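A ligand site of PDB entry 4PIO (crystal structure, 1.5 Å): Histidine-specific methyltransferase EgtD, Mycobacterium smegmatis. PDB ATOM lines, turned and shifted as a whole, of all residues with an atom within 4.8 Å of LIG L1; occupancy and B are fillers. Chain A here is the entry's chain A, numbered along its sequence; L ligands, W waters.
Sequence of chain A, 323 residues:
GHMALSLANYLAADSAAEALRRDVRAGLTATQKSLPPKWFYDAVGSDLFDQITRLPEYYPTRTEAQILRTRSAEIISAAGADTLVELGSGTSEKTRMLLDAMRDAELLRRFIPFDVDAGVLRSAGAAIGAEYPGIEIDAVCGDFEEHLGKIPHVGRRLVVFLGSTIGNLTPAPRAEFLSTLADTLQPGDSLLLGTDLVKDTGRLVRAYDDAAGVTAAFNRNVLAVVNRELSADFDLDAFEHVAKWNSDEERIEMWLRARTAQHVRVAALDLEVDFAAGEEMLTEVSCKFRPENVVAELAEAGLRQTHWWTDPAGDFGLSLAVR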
ATOM      1  N   LYS A  38       1.676 -30.899   0.944  1.00  0.00           N
ATOM      2  CA  LYS A  38       0.464 -31.470   0.334  1.00  0.00           C
ATOM      3  C   LYS A  38       0.386 -32.969   0.604  1.00  0.00           C
ATOM      4  O   LYS A  38      -0.696 -33.547   0.693  1.00  0.00           O
ATOM      5  CB  LYS A  38       0.404 -31.219  -1.172  1.00  0.00           C
ATOM      6  CG  LYS A  38       1.454 -31.950  -1.956  1.00  0.00           C
ATOM      7  CD  LYS A  38       1.479 -31.539  -3.436  1.00  0.00           C
ATOM      8  CE  LYS A  38       0.568 -32.358  -4.289  1.00  0.00           C
ATOM      9  NZ  LYS A  38       0.881 -32.121  -5.746  1.00  0.00           N
ATOM     10  N   TYR A  41      -1.615 -35.195   3.527  1.00  0.00           N
ATOM     11  CA  TYR A  41      -3.059 -35.386   3.548  1.00  0.00           C
ATOM     12  C   TYR A  41      -3.509 -36.639   2.789  1.00  0.00           C
ATOM     13  O   TYR A  41      -4.228 -36.562   1.795  1.00  0.00           O
ATOM     14  CB  TYR A  41      -3.759 -34.141   2.995  1.00  0.00           C
ATOM     15  CG  TYR A  41      -3.423 -32.899   3.773  1.00  0.00           C
ATOM     16  CD1 TYR A  41      -4.105 -32.568   4.923  1.00  0.00           C
ATOM     17  CD2 TYR A  41      -2.387 -32.062   3.367  1.00  0.00           C
ATOM     18  CE1 TYR A  41      -3.795 -31.431   5.643  1.00  0.00           C
ATOM     19  CE2 TYR A  41      -2.073 -30.935   4.065  1.00  0.00           C
ATOM     20  CZ  TYR A  41      -2.770 -30.623   5.213  1.00  0.00           C
ATOM     21  OH  TYR A  41      -2.470 -29.483   5.935  1.00  0.00           O
ATOM     22  N   SER A  46      -5.351 -36.580   6.935  1.00  0.00           N
ATOM     23  CA  SER A  46      -6.546 -35.734   6.927  1.00  0.00           C
ATOM     24  C   SER A  46      -7.291 -35.888   8.227  1.00  0.00           C
ATOM     25  O   SER A  46      -7.811 -34.921   8.771  1.00  0.00           O
ATOM     26  CB  SER A  46      -7.433 -36.064   5.736  1.00  0.00           C
ATOM     27  OG  SER A  46      -6.871 -35.538   4.547  1.00  0.00           O
ATOM     28  N   PHE A  49      -5.308 -34.066  10.913  1.00  0.00           N
ATOM     29  CA  PHE A  49      -5.542 -32.637  10.836  1.00  0.00           C
ATOM     30  C   PHE A  49      -6.912 -32.307  11.443  1.00  0.00           C
ATOM     31  O   PHE A  49      -7.044 -31.330  12.182  1.00  0.00           O
ATOM     32  CB  PHE A  49      -5.502 -32.076   9.412  1.00  0.00           C
ATOM     33  CG  PHE A  49      -5.788 -30.612   9.402  1.00  0.00           C
ATOM     34  CD1 PHE A  49      -4.807 -29.710   9.781  1.00  0.00           C
ATOM     35  CD2 PHE A  49      -7.076 -30.135   9.163  1.00  0.00           C
ATOM     36  CE1 PHE A  49      -5.081 -28.367   9.866  1.00  0.00           C
ATOM     37  CE2 PHE A  49      -7.347 -28.785   9.254  1.00  0.00           C
ATOM     38  CZ  PHE A  49      -6.355 -27.904   9.603  1.00  0.00           C
ATOM     39  N   THR A  53      -7.671 -29.585  14.689  1.00  0.00           N
ATOM     40  CA  THR A  53      -8.567 -28.427  14.711  1.00  0.00           C
ATOM     41  C   THR A  53      -9.272 -28.263  16.048  1.00  0.00           C
ATOM     42  O   THR A  53      -9.818 -27.199  16.298  1.00  0.00           O
ATOM     43  CB  THR A  53      -9.644 -28.474  13.597  1.00  0.00           C
ATOM     44  OG1 THR A  53     -10.618 -29.491  13.844  1.00  0.00           O
ATOM     45  CG2 THR A  53      -9.015 -28.662  12.228  1.00  0.00           C
ATOM     46  N   THR A  61      -8.723 -22.772  13.993  1.00  0.00           N
ATOM     47  CA  THR A  61     -10.008 -23.224  13.506  1.00  0.00           C
ATOM     48  C   THR A  61     -11.142 -22.560  14.263  1.00  0.00           C
ATOM     49  O   THR A  61     -12.078 -22.051  13.659  1.00  0.00           O
ATOM     50  CB  THR A  61     -10.135 -24.756  13.622  1.00  0.00           C
ATOM     51  OG1 THR A  61      -8.958 -25.392  13.092  1.00  0.00           O
ATOM     52  CG2 THR A  61     -11.368 -25.221  12.840  1.00  0.00           C
ATOM     53  N   GLU A  64     -11.415 -18.742  13.401  1.00  0.00           N
ATOM     54  CA  GLU A  64     -12.033 -18.458  12.098  1.00  0.00           C
ATOM     55  C   GLU A  64     -13.505 -18.849  12.112  1.00  0.00           C
ATOM     56  O   GLU A  64     -14.359 -18.181  11.520  1.00  0.00           O
ATOM     57  CB  GLU A  64     -11.289 -19.164  10.966  1.00  0.00           C
ATOM     58  CG  GLU A  64     -11.841 -18.839   9.578  1.00  0.00           C
ATOM     59  CD  GLU A  64     -11.050 -19.507   8.476  1.00  0.00           C
ATOM     60  OE1 GLU A  64     -10.717 -20.702   8.613  1.00  0.00           O
ATOM     61  OE2 GLU A  64     -10.748 -18.859   7.466  1.00  0.00           O
ATOM     62  N   GLU A  86     -14.898 -24.272  -2.710  1.00  0.00           N
ATOM     63  CA  GLU A  86     -13.969 -24.243  -1.582  1.00  0.00           C
ATOM     64  C   GLU A  86     -12.637 -24.935  -1.902  1.00  0.00           C
ATOM     65  O   GLU A  86     -12.600 -26.105  -2.269  1.00  0.00           O
ATOM     66  CB  GLU A  86     -14.557 -24.894  -0.326  1.00  0.00           C
ATOM     67  CG  GLU A  86     -13.616 -24.716   0.844  1.00  0.00           C
ATOM     68  CD  GLU A  86     -14.145 -25.187   2.181  1.00  0.00           C
ATOM     69  OE1 GLU A  86     -15.163 -25.914   2.239  1.00  0.00           O
ATOM     70  OE2 GLU A  86     -13.509 -24.816   3.177  1.00  0.00           O
ATOM     71  N   GLY A  88      -9.012 -26.488  -0.830  1.00  0.00           N
ATOM     72  CA  GLY A  88      -8.461 -27.161   0.340  1.00  0.00           C
ATOM     73  C   GLY A  88      -9.560 -27.373   1.354  1.00  0.00           C
ATOM     74  O   GLY A  88      -9.437 -27.018   2.525  1.00  0.00           O
ATOM     75  N   SER A  89     -10.659 -27.942   0.886  1.00  0.00           N
ATOM     76  CA  SER A  89     -11.902 -27.942   1.623  1.00  0.00           C
ATOM     77  C   SER A  89     -11.930 -28.884   2.829  1.00  0.00           C
ATOM     78  O   SER A  89     -12.613 -28.627   3.804  1.00  0.00           O
ATOM     79  CB  SER A  89     -13.023 -28.284   0.631  1.00  0.00           C
ATOM     80  OG  SER A  89     -12.746 -29.521  -0.023  1.00  0.00           O
ATOM     81  N   GLY A  90     -11.184 -29.980   2.770  1.00  0.00           N
ATOM     82  CA  GLY A  90     -11.166 -30.927   3.895  1.00  0.00           C
ATOM     83  C   GLY A  90     -12.561 -31.413   4.242  1.00  0.00           C
ATOM     84  O   GLY A  90     -13.285 -31.846   3.351  1.00  0.00           O
ATOM     85  N   LYS A  94     -16.519 -25.915   8.732  1.00  0.00           N
ATOM     86  CA  LYS A  94     -16.751 -24.492   8.881  1.00  0.00           C
ATOM     87  C   LYS A  94     -17.644 -23.968   7.749  1.00  0.00           C
ATOM     88  O   LYS A  94     -18.428 -23.046   7.926  1.00  0.00           O
ATOM     89  CB  LYS A  94     -15.420 -23.754   8.904  1.00  0.00           C
ATOM     90  CG  LYS A  94     -14.611 -23.927  10.192  1.00  0.00           C
ATOM     91  CD  LYS A  94     -13.257 -23.198  10.131  1.00  0.00           C
ATOM     92  CE  LYS A  94     -12.290 -23.849   9.155  1.00  0.00           C
ATOM     93  NZ  LYS A  94     -10.974 -23.148   9.149  1.00  0.00           N
ATOM     94  N   PHE A 114     -12.779 -28.636  -3.510  1.00  0.00           N
ATOM     95  CA  PHE A 114     -11.547 -28.853  -4.255  1.00  0.00           C
ATOM     96  C   PHE A 114     -10.488 -29.275  -3.249  1.00  0.00           C
ATOM     97  O   PHE A 114     -10.257 -28.567  -2.271  1.00  0.00           O
ATOM     98  CB  PHE A 114     -11.127 -27.588  -4.988  1.00  0.00           C
ATOM     99  CG  PHE A 114      -9.849 -27.741  -5.786  1.00  0.00           C
ATOM    100  CD1 PHE A 114      -8.619 -27.683  -5.165  1.00  0.00           C
ATOM    101  CD2 PHE A 114      -9.882 -27.881  -7.170  1.00  0.00           C
ATOM    102  CE1 PHE A 114      -7.440 -27.790  -5.886  1.00  0.00           C
ATOM    103  CE2 PHE A 114      -8.706 -27.990  -7.904  1.00  0.00           C
ATOM    104  CZ  PHE A 114      -7.485 -27.948  -7.258  1.00  0.00           C
ATOM    105  N   ASP A 115      -9.857 -30.424  -3.453  1.00  0.00           N
ATOM    106  CA  ASP A 115      -8.891 -30.911  -2.471  1.00  0.00           C
ATOM    107  C   ASP A 115      -7.977 -31.944  -3.112  1.00  0.00           C
ATOM    108  O   ASP A 115      -8.336 -32.561  -4.106  1.00  0.00           O
ATOM    109  CB  ASP A 115      -9.609 -31.540  -1.260  1.00  0.00           C
ATOM    110  CG  ASP A 115      -8.763 -31.529  -0.004  1.00  0.00           C
ATOM    111  OD1 ASP A 115      -7.872 -32.384   0.167  1.00  0.00           O
ATOM    112  OD2 ASP A 115      -9.005 -30.623   0.846  1.00  0.00           O
ATOM    113  N   VAL A 116      -6.811 -32.118  -2.537  1.00  0.00           N
ATOM    114  CA  VAL A 116      -5.857 -33.110  -3.030  1.00  0.00           C
ATOM    115  C   VAL A 116      -6.232 -34.523  -2.570  1.00  0.00           C
ATOM    116  O   VAL A 116      -5.828 -35.512  -3.194  1.00  0.00           O
ATOM    117  CB  VAL A 116      -4.421 -32.751  -2.568  1.00  0.00           C
ATOM    118  CG1 VAL A 116      -4.246 -32.909  -1.067  1.00  0.00           C
ATOM    119  CG2 VAL A 116      -3.397 -33.574  -3.324  1.00  0.00           C
ATOM    120  N   ASP A 117      -7.024 -34.625  -1.511  1.00  0.00           N
ATOM    121  CA  ASP A 117      -7.355 -35.902  -0.891  1.00  0.00           C
ATOM    122  C   ASP A 117      -8.738 -36.351  -1.349  1.00  0.00           C
ATOM    123  O   ASP A 117      -9.739 -35.816  -0.916  1.00  0.00           O
ATOM    124  CB  ASP A 117      -7.288 -35.780   0.633  1.00  0.00           C
ATOM    125  CG  ASP A 117      -7.759 -37.040   1.370  1.00  0.00           C
ATOM    126  OD1 ASP A 117      -7.957 -38.101   0.749  1.00  0.00           O
ATOM    127  OD2 ASP A 117      -7.904 -36.955   2.610  1.00  0.00           O
ATOM    128  N   VAL A 120     -11.441 -37.280   1.359  1.00  0.00           N
ATOM    129  CA  VAL A 120     -12.137 -36.275   2.127  1.00  0.00           C
ATOM    130  C   VAL A 120     -13.209 -35.615   1.249  1.00  0.00           C
ATOM    131  O   VAL A 120     -14.266 -35.235   1.738  1.00  0.00           O
ATOM    132  CB  VAL A 120     -11.122 -35.248   2.735  1.00  0.00           C
ATOM    133  CG1 VAL A 120     -10.883 -34.058   1.816  1.00  0.00           C
ATOM    134  CG2 VAL A 120     -11.596 -34.801   4.105  1.00  0.00           C
ATOM    135  N   GLY A 142      -7.495 -32.229  -6.984  1.00  0.00           N
ATOM    136  CA  GLY A 142      -6.336 -31.626  -7.594  1.00  0.00           C
ATOM    137  C   GLY A 142      -5.493 -30.869  -6.598  1.00  0.00           C
ATOM    138  O   GLY A 142      -5.799 -30.800  -5.407  1.00  0.00           O
ATOM    139  N   ASP A 143      -4.416 -30.282  -7.129  1.00  0.00           N
ATOM    140  CA  ASP A 143      -3.450 -29.471  -6.412  1.00  0.00           C
ATOM    141  C   ASP A 143      -3.782 -27.999  -6.711  1.00  0.00           C
ATOM    142  O   ASP A 143      -3.825 -27.613  -7.876  1.00  0.00           O
ATOM    143  CB  ASP A 143      -2.032 -29.850  -6.880  1.00  0.00           C
ATOM    144  CG  ASP A 143      -0.927 -29.037  -6.201  1.00  0.00           C
ATOM    145  OD1 ASP A 143      -1.156 -27.942  -5.662  1.00  0.00           O
ATOM    146  OD2 ASP A 143       0.235 -29.502  -6.233  1.00  0.00           O
ATOM    147  N   PHE A 144      -4.019 -27.181  -5.688  1.00  0.00           N
ATOM    148  CA  PHE A 144      -4.489 -25.823  -5.960  1.00  0.00           C
ATOM    149  C   PHE A 144      -3.399 -24.942  -6.564  1.00  0.00           C
ATOM    150  O   PHE A 144      -3.688 -23.845  -7.037  1.00  0.00           O
ATOM    151  CB  PHE A 144      -5.122 -25.140  -4.720  1.00  0.00           C
ATOM    152  CG  PHE A 144      -4.347 -25.227  -3.440  1.00  0.00           C
ATOM    153  CD1 PHE A 144      -3.045 -24.758  -3.350  1.00  0.00           C
ATOM    154  CD2 PHE A 144      -4.953 -25.735  -2.286  1.00  0.00           C
ATOM    155  CE1 PHE A 144      -2.355 -24.836  -2.139  1.00  0.00           C
ATOM    156  CE2 PHE A 144      -4.273 -25.792  -1.095  1.00  0.00           C
ATOM    157  CZ  PHE A 144      -2.980 -25.358  -1.008  1.00  0.00           C
ATOM    158  N   LEU A 162     -10.226 -21.159   3.291  1.00  0.00           N
ATOM    159  CA  LEU A 162     -10.188 -20.955   4.727  1.00  0.00           C
ATOM    160  C   LEU A 162      -8.926 -21.496   5.377  1.00  0.00           C
ATOM    161  O   LEU A 162      -8.087 -22.141   4.742  1.00  0.00           O
ATOM    162  CB  LEU A 162     -11.377 -21.646   5.395  1.00  0.00           C
ATOM    163  CG  LEU A 162     -12.778 -21.301   4.909  1.00  0.00           C
ATOM    164  CD1 LEU A 162     -13.765 -22.140   5.711  1.00  0.00           C
ATOM    165  CD2 LEU A 162     -13.065 -19.826   5.036  1.00  0.00           C
ATOM    166  N   GLY A 163      -8.782 -21.196   6.657  1.00  0.00           N
ATOM    167  CA  GLY A 163      -7.836 -21.927   7.467  1.00  0.00           C
ATOM    168  C   GLY A 163      -6.421 -21.404   7.483  1.00  0.00           C
ATOM    169  O   GLY A 163      -5.580 -21.922   8.197  1.00  0.00           O
ATOM    170  N   THR A 165      -4.587 -21.805   4.975  1.00  0.00           N
ATOM    171  CA  THR A 165      -3.871 -22.725   4.108  1.00  0.00           C
ATOM    172  C   THR A 165      -3.056 -21.931   3.079  1.00  0.00           C
ATOM    173  O   THR A 165      -2.047 -22.412   2.573  1.00  0.00           O
ATOM    174  CB  THR A 165      -4.839 -23.707   3.471  1.00  0.00           C
ATOM    175  OG1 THR A 165      -5.501 -24.412   4.531  1.00  0.00           O
ATOM    176  CG2 THR A 165      -4.127 -24.710   2.575  1.00  0.00           C
HETATM  177  N1  LIG L   1     -10.335 -26.150   4.972  1.00  0.00           N
HETATM  178  C1  LIG L   1     -10.148 -26.915   6.203  1.00  0.00           C
HETATM  179  C2  LIG L   1      -8.953 -27.866   6.074  1.00  0.00           C
HETATM  180  C3  LIG L   1      -7.595 -27.197   6.054  1.00  0.00           C
HETATM  181  S1  LIG L   1      -6.243 -28.397   6.107  1.00  0.00           S
HETATM  182  C4  LIG L   1      -9.936 -25.979   7.391  1.00  0.00           C
HETATM  183  O1  LIG L   1      -9.905 -26.413   8.505  1.00  0.00           O
HETATM  184  O2  LIG L   1      -9.826 -24.679   7.153  1.00  0.00           O
HETATM  185  C5  LIG L   1      -5.685 -28.193   4.401  1.00  0.00           C
HETATM  186  C6  LIG L   1      -6.631 -28.831   3.374  1.00  0.00           C
HETATM  187  O3  LIG L   1      -6.174 -28.547   2.054  1.00  0.00           O
HETATM  188  C7  LIG L   1      -6.721 -30.353   3.510  1.00  0.00           C
HETATM  189  O4  LIG L   1      -8.025 -30.853   3.292  1.00  0.00           O
HETATM  190  C8  LIG L   1      -5.714 -30.818   2.465  1.00  0.00           C
HETATM  191  O5  LIG L   1      -5.916 -32.125   1.954  1.00  0.00           O
HETATM  192  C9  LIG L   1      -5.822 -29.759   1.381  1.00  0.00           C
HETATM  193  N2  LIG L   1      -4.589 -29.462   0.664  1.00  0.00           N
HETATM  194  C10 LIG L   1      -3.356 -29.232   1.153  1.00  0.00           C
HETATM  195  N3  LIG L   1      -2.525 -28.919   0.147  1.00  0.00           N
HETATM  196  C11 LIG L   1      -3.242 -28.897  -0.981  1.00  0.00           C
HETATM  197  C12 LIG L   1      -2.930 -28.643  -2.309  1.00  0.00           C
HETATM  198  N4  LIG L   1      -1.689 -28.321  -2.710  1.00  0.00           N
HETATM  199  N5  LIG L   1      -3.940 -28.720  -3.218  1.00  0.00           N
HETATM  200  C13 LIG L   1      -5.228 -29.049  -2.886  1.00  0.00           C
HETATM  201  N6  LIG L   1      -5.533 -29.307  -1.573  1.00  0.00           N
HETATM  202  C14 LIG L   1      -4.551 -29.247  -0.679  1.00  0.00           C
HETATM  203  C1  LG2 L   2      -3.703 -26.276   6.868  1.00  0.00           C
HETATM  204  N1  LG2 L   2      -2.788 -25.272   7.370  1.00  0.00           N
HETATM  205  C2  LG2 L   2      -3.624 -24.096   7.508  1.00  0.00           C
HETATM  206  C3  LG2 L   2      -2.350 -25.676   8.695  1.00  0.00           C
HETATM  207  C4  LG2 L   2      -1.520 -24.589   9.354  1.00  0.00           C
HETATM  208  O1  LG2 L   2      -0.580 -24.247   8.743  1.00  0.00           O
HETATM  209  O2  LG2 L   2      -1.945 -24.162  10.423  1.00  0.00           O
HETATM  210  C5  LG2 L   2      -1.574 -26.984   8.669  1.00  0.00           C
HETATM  211  C6  LG2 L   2      -1.028 -27.424  10.002  1.00  0.00           C
HETATM  212  N2  LG2 L   2       0.205 -27.885  10.165  1.00  0.00           N
HETATM  213  C7  LG2 L   2       0.407 -28.181  11.440  1.00  0.00           C
HETATM  214  N3  LG2 L   2      -0.693 -27.915  12.107  1.00  0.00           N
HETATM  215  C8  LG2 L   2      -1.614 -27.454  11.220  1.00  0.00           C
HETATM  216  O   HOH W   1      -8.073 -24.679   3.582  1.00  0.00           O
HETATM  217  O   HOH W   2     -10.812 -30.513   7.358  1.00  0.00           O
HETATM  218  O   HOH W   3      -0.230 -27.841   1.780  1.00  0.00           O
HETATM  219  O   HOH W   4     -11.013 -23.868   2.660  1.00  0.00           O
HETATM  220  O   HOH W   5      -8.848 -24.816  10.458  1.00  0.00           O
HETATM  221  O   HOH W   6     -11.872 -27.994   9.314  1.00  0.00           O
HETATM  222  O   HOH W   7     -13.184 -26.362   5.215  1.00  0.00           O
HETATM  223  O   HOH W   8       0.819 -27.192  -1.733  1.00  0.00           O
HETATM  224  O   HOH W   9      -8.236 -33.107   4.805  1.00  0.00           O
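The backbone carbonyl oxygen (O) of Gly 142 sits close to the backbone NH (N) of Val 116 (3.3 Å). The backbone carbonyl oxygen of Phe 114 is in hydrogen-bond range of the backbone NH of Gly 88 (2.8 Å). The side-chain amino group of Lys 38 lies within salt-bridge range of the side-chain carboxylate of Asp 143. The side-chain carboxylate (OE1) of Glu 64 is in hydrogen-bond range of the backbone NH (N) of Gly 163 (2.8 Å). The side-chain amino group (NZ) of Lys 94 lies within salt-bridge range of the side-chain carboxylate (OE1) of Glu 64, 2.5 Å away. The backbone NH (N) of Gly 90 sits at hydrogen-bond distance from the side-chain carboxylate (OD2) of Asp 115, at 3.0 Å. The side-chain carboxylate (OD2) of Asp 115 sits at hydrogen-bond distance from the backbone NH (N) of Ser 89 (3.2 Å). N of Phe 114 sits at hydrogen-bond distance from O of Glu 86 (2.8 Å).
OD2 of Asp 115 lies within hydrogen-bond range of O4 of LIG L1, at 2.6 Å. O4 of LIG L1 sits close to N of Gly 90. A nitrogen (N5) of LIG L1 sits at hydrogen-bond distance from the backbone NH of Phe 144 (2.9 Å). A nitrogen (N1) of LIG L1 sits at hydrogen-bond distance from the backbone carbonyl oxygen (O) of Gly 88 (2.7 Å). The backbone NH (N) of Val 116 is in hydrogen-bond range of a nitrogen (N6) of LIG L1 (3.2 Å). OD1 of Asp 143 is in hydrogen-bond range of N4 of LIG L1, 3.0 Å away. An oxygen (O2) of LIG L1 lies within salt-bridge range of the side-chain amino group (NZ) of Lys 94 (2.8 Å). The side-chain carboxylate (OE2) of Glu 86 is in salt-bridge range of a nitrogen (N1) of LIG L1, at 3.9 Å.
Water W9 bridges an oxygen (O4) of LIG L1 and the side-chain hydroxyl of Ser 46. Water W5 lies within hydrogen-bond range of OG1 of Thr 61 (2.7 Å), O1 of LIG L1 (2.7 Å) and NZ of Lys 94 (3.0 Å). Water W7 lies within hydrogen-bond range of the side-chain carboxylate of Glu 86, the backbone carbonyl oxygen of Ser 89 and a nitrogen (N1) of LIG L1. Water W1 lies within hydrogen-bond range of the side-chain hydroxyl of Thr 165 (2.8 Å), the backbone carbonyl oxygen of Leu 162 (2.8 Å), the backbone carbonyl oxygen of Gly 88 (2.9 Å) and a nitrogen (N1) of LIG L1 (3.0 Å). Water W4 lies within hydrogen-bond range of the side-chain carboxylate of Glu 86 (2.7 Å), the backbone NH of Leu 162 (2.9 Å) and a nitrogen (N1) of LIG L1 (3.3 Å).
Merely in contact with LIG L1: Lys 38 (3.9 Å), Tyr 41 (3.1 Å), Phe 49 (3.4 Å), Ser 89 (3.6 Å), Phe 114 (3.9 Å), Gly 142 (3.1 Å), Leu 162 (3.8 Å), Gly 163 (3.4 Å) and Thr 165 (3.8 Å). Hydrophobic or aromatic side chains that line LIG L1: Tyr 41, Phe 49, Phe 114, Val 116, Phe 144 and Leu 162. Along chain A the residues within 4 Å of LIG L1 span positions 38 to 165. The nearest printed residue that does not touch LIG L1 is Asp 117 (4.1 Å).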
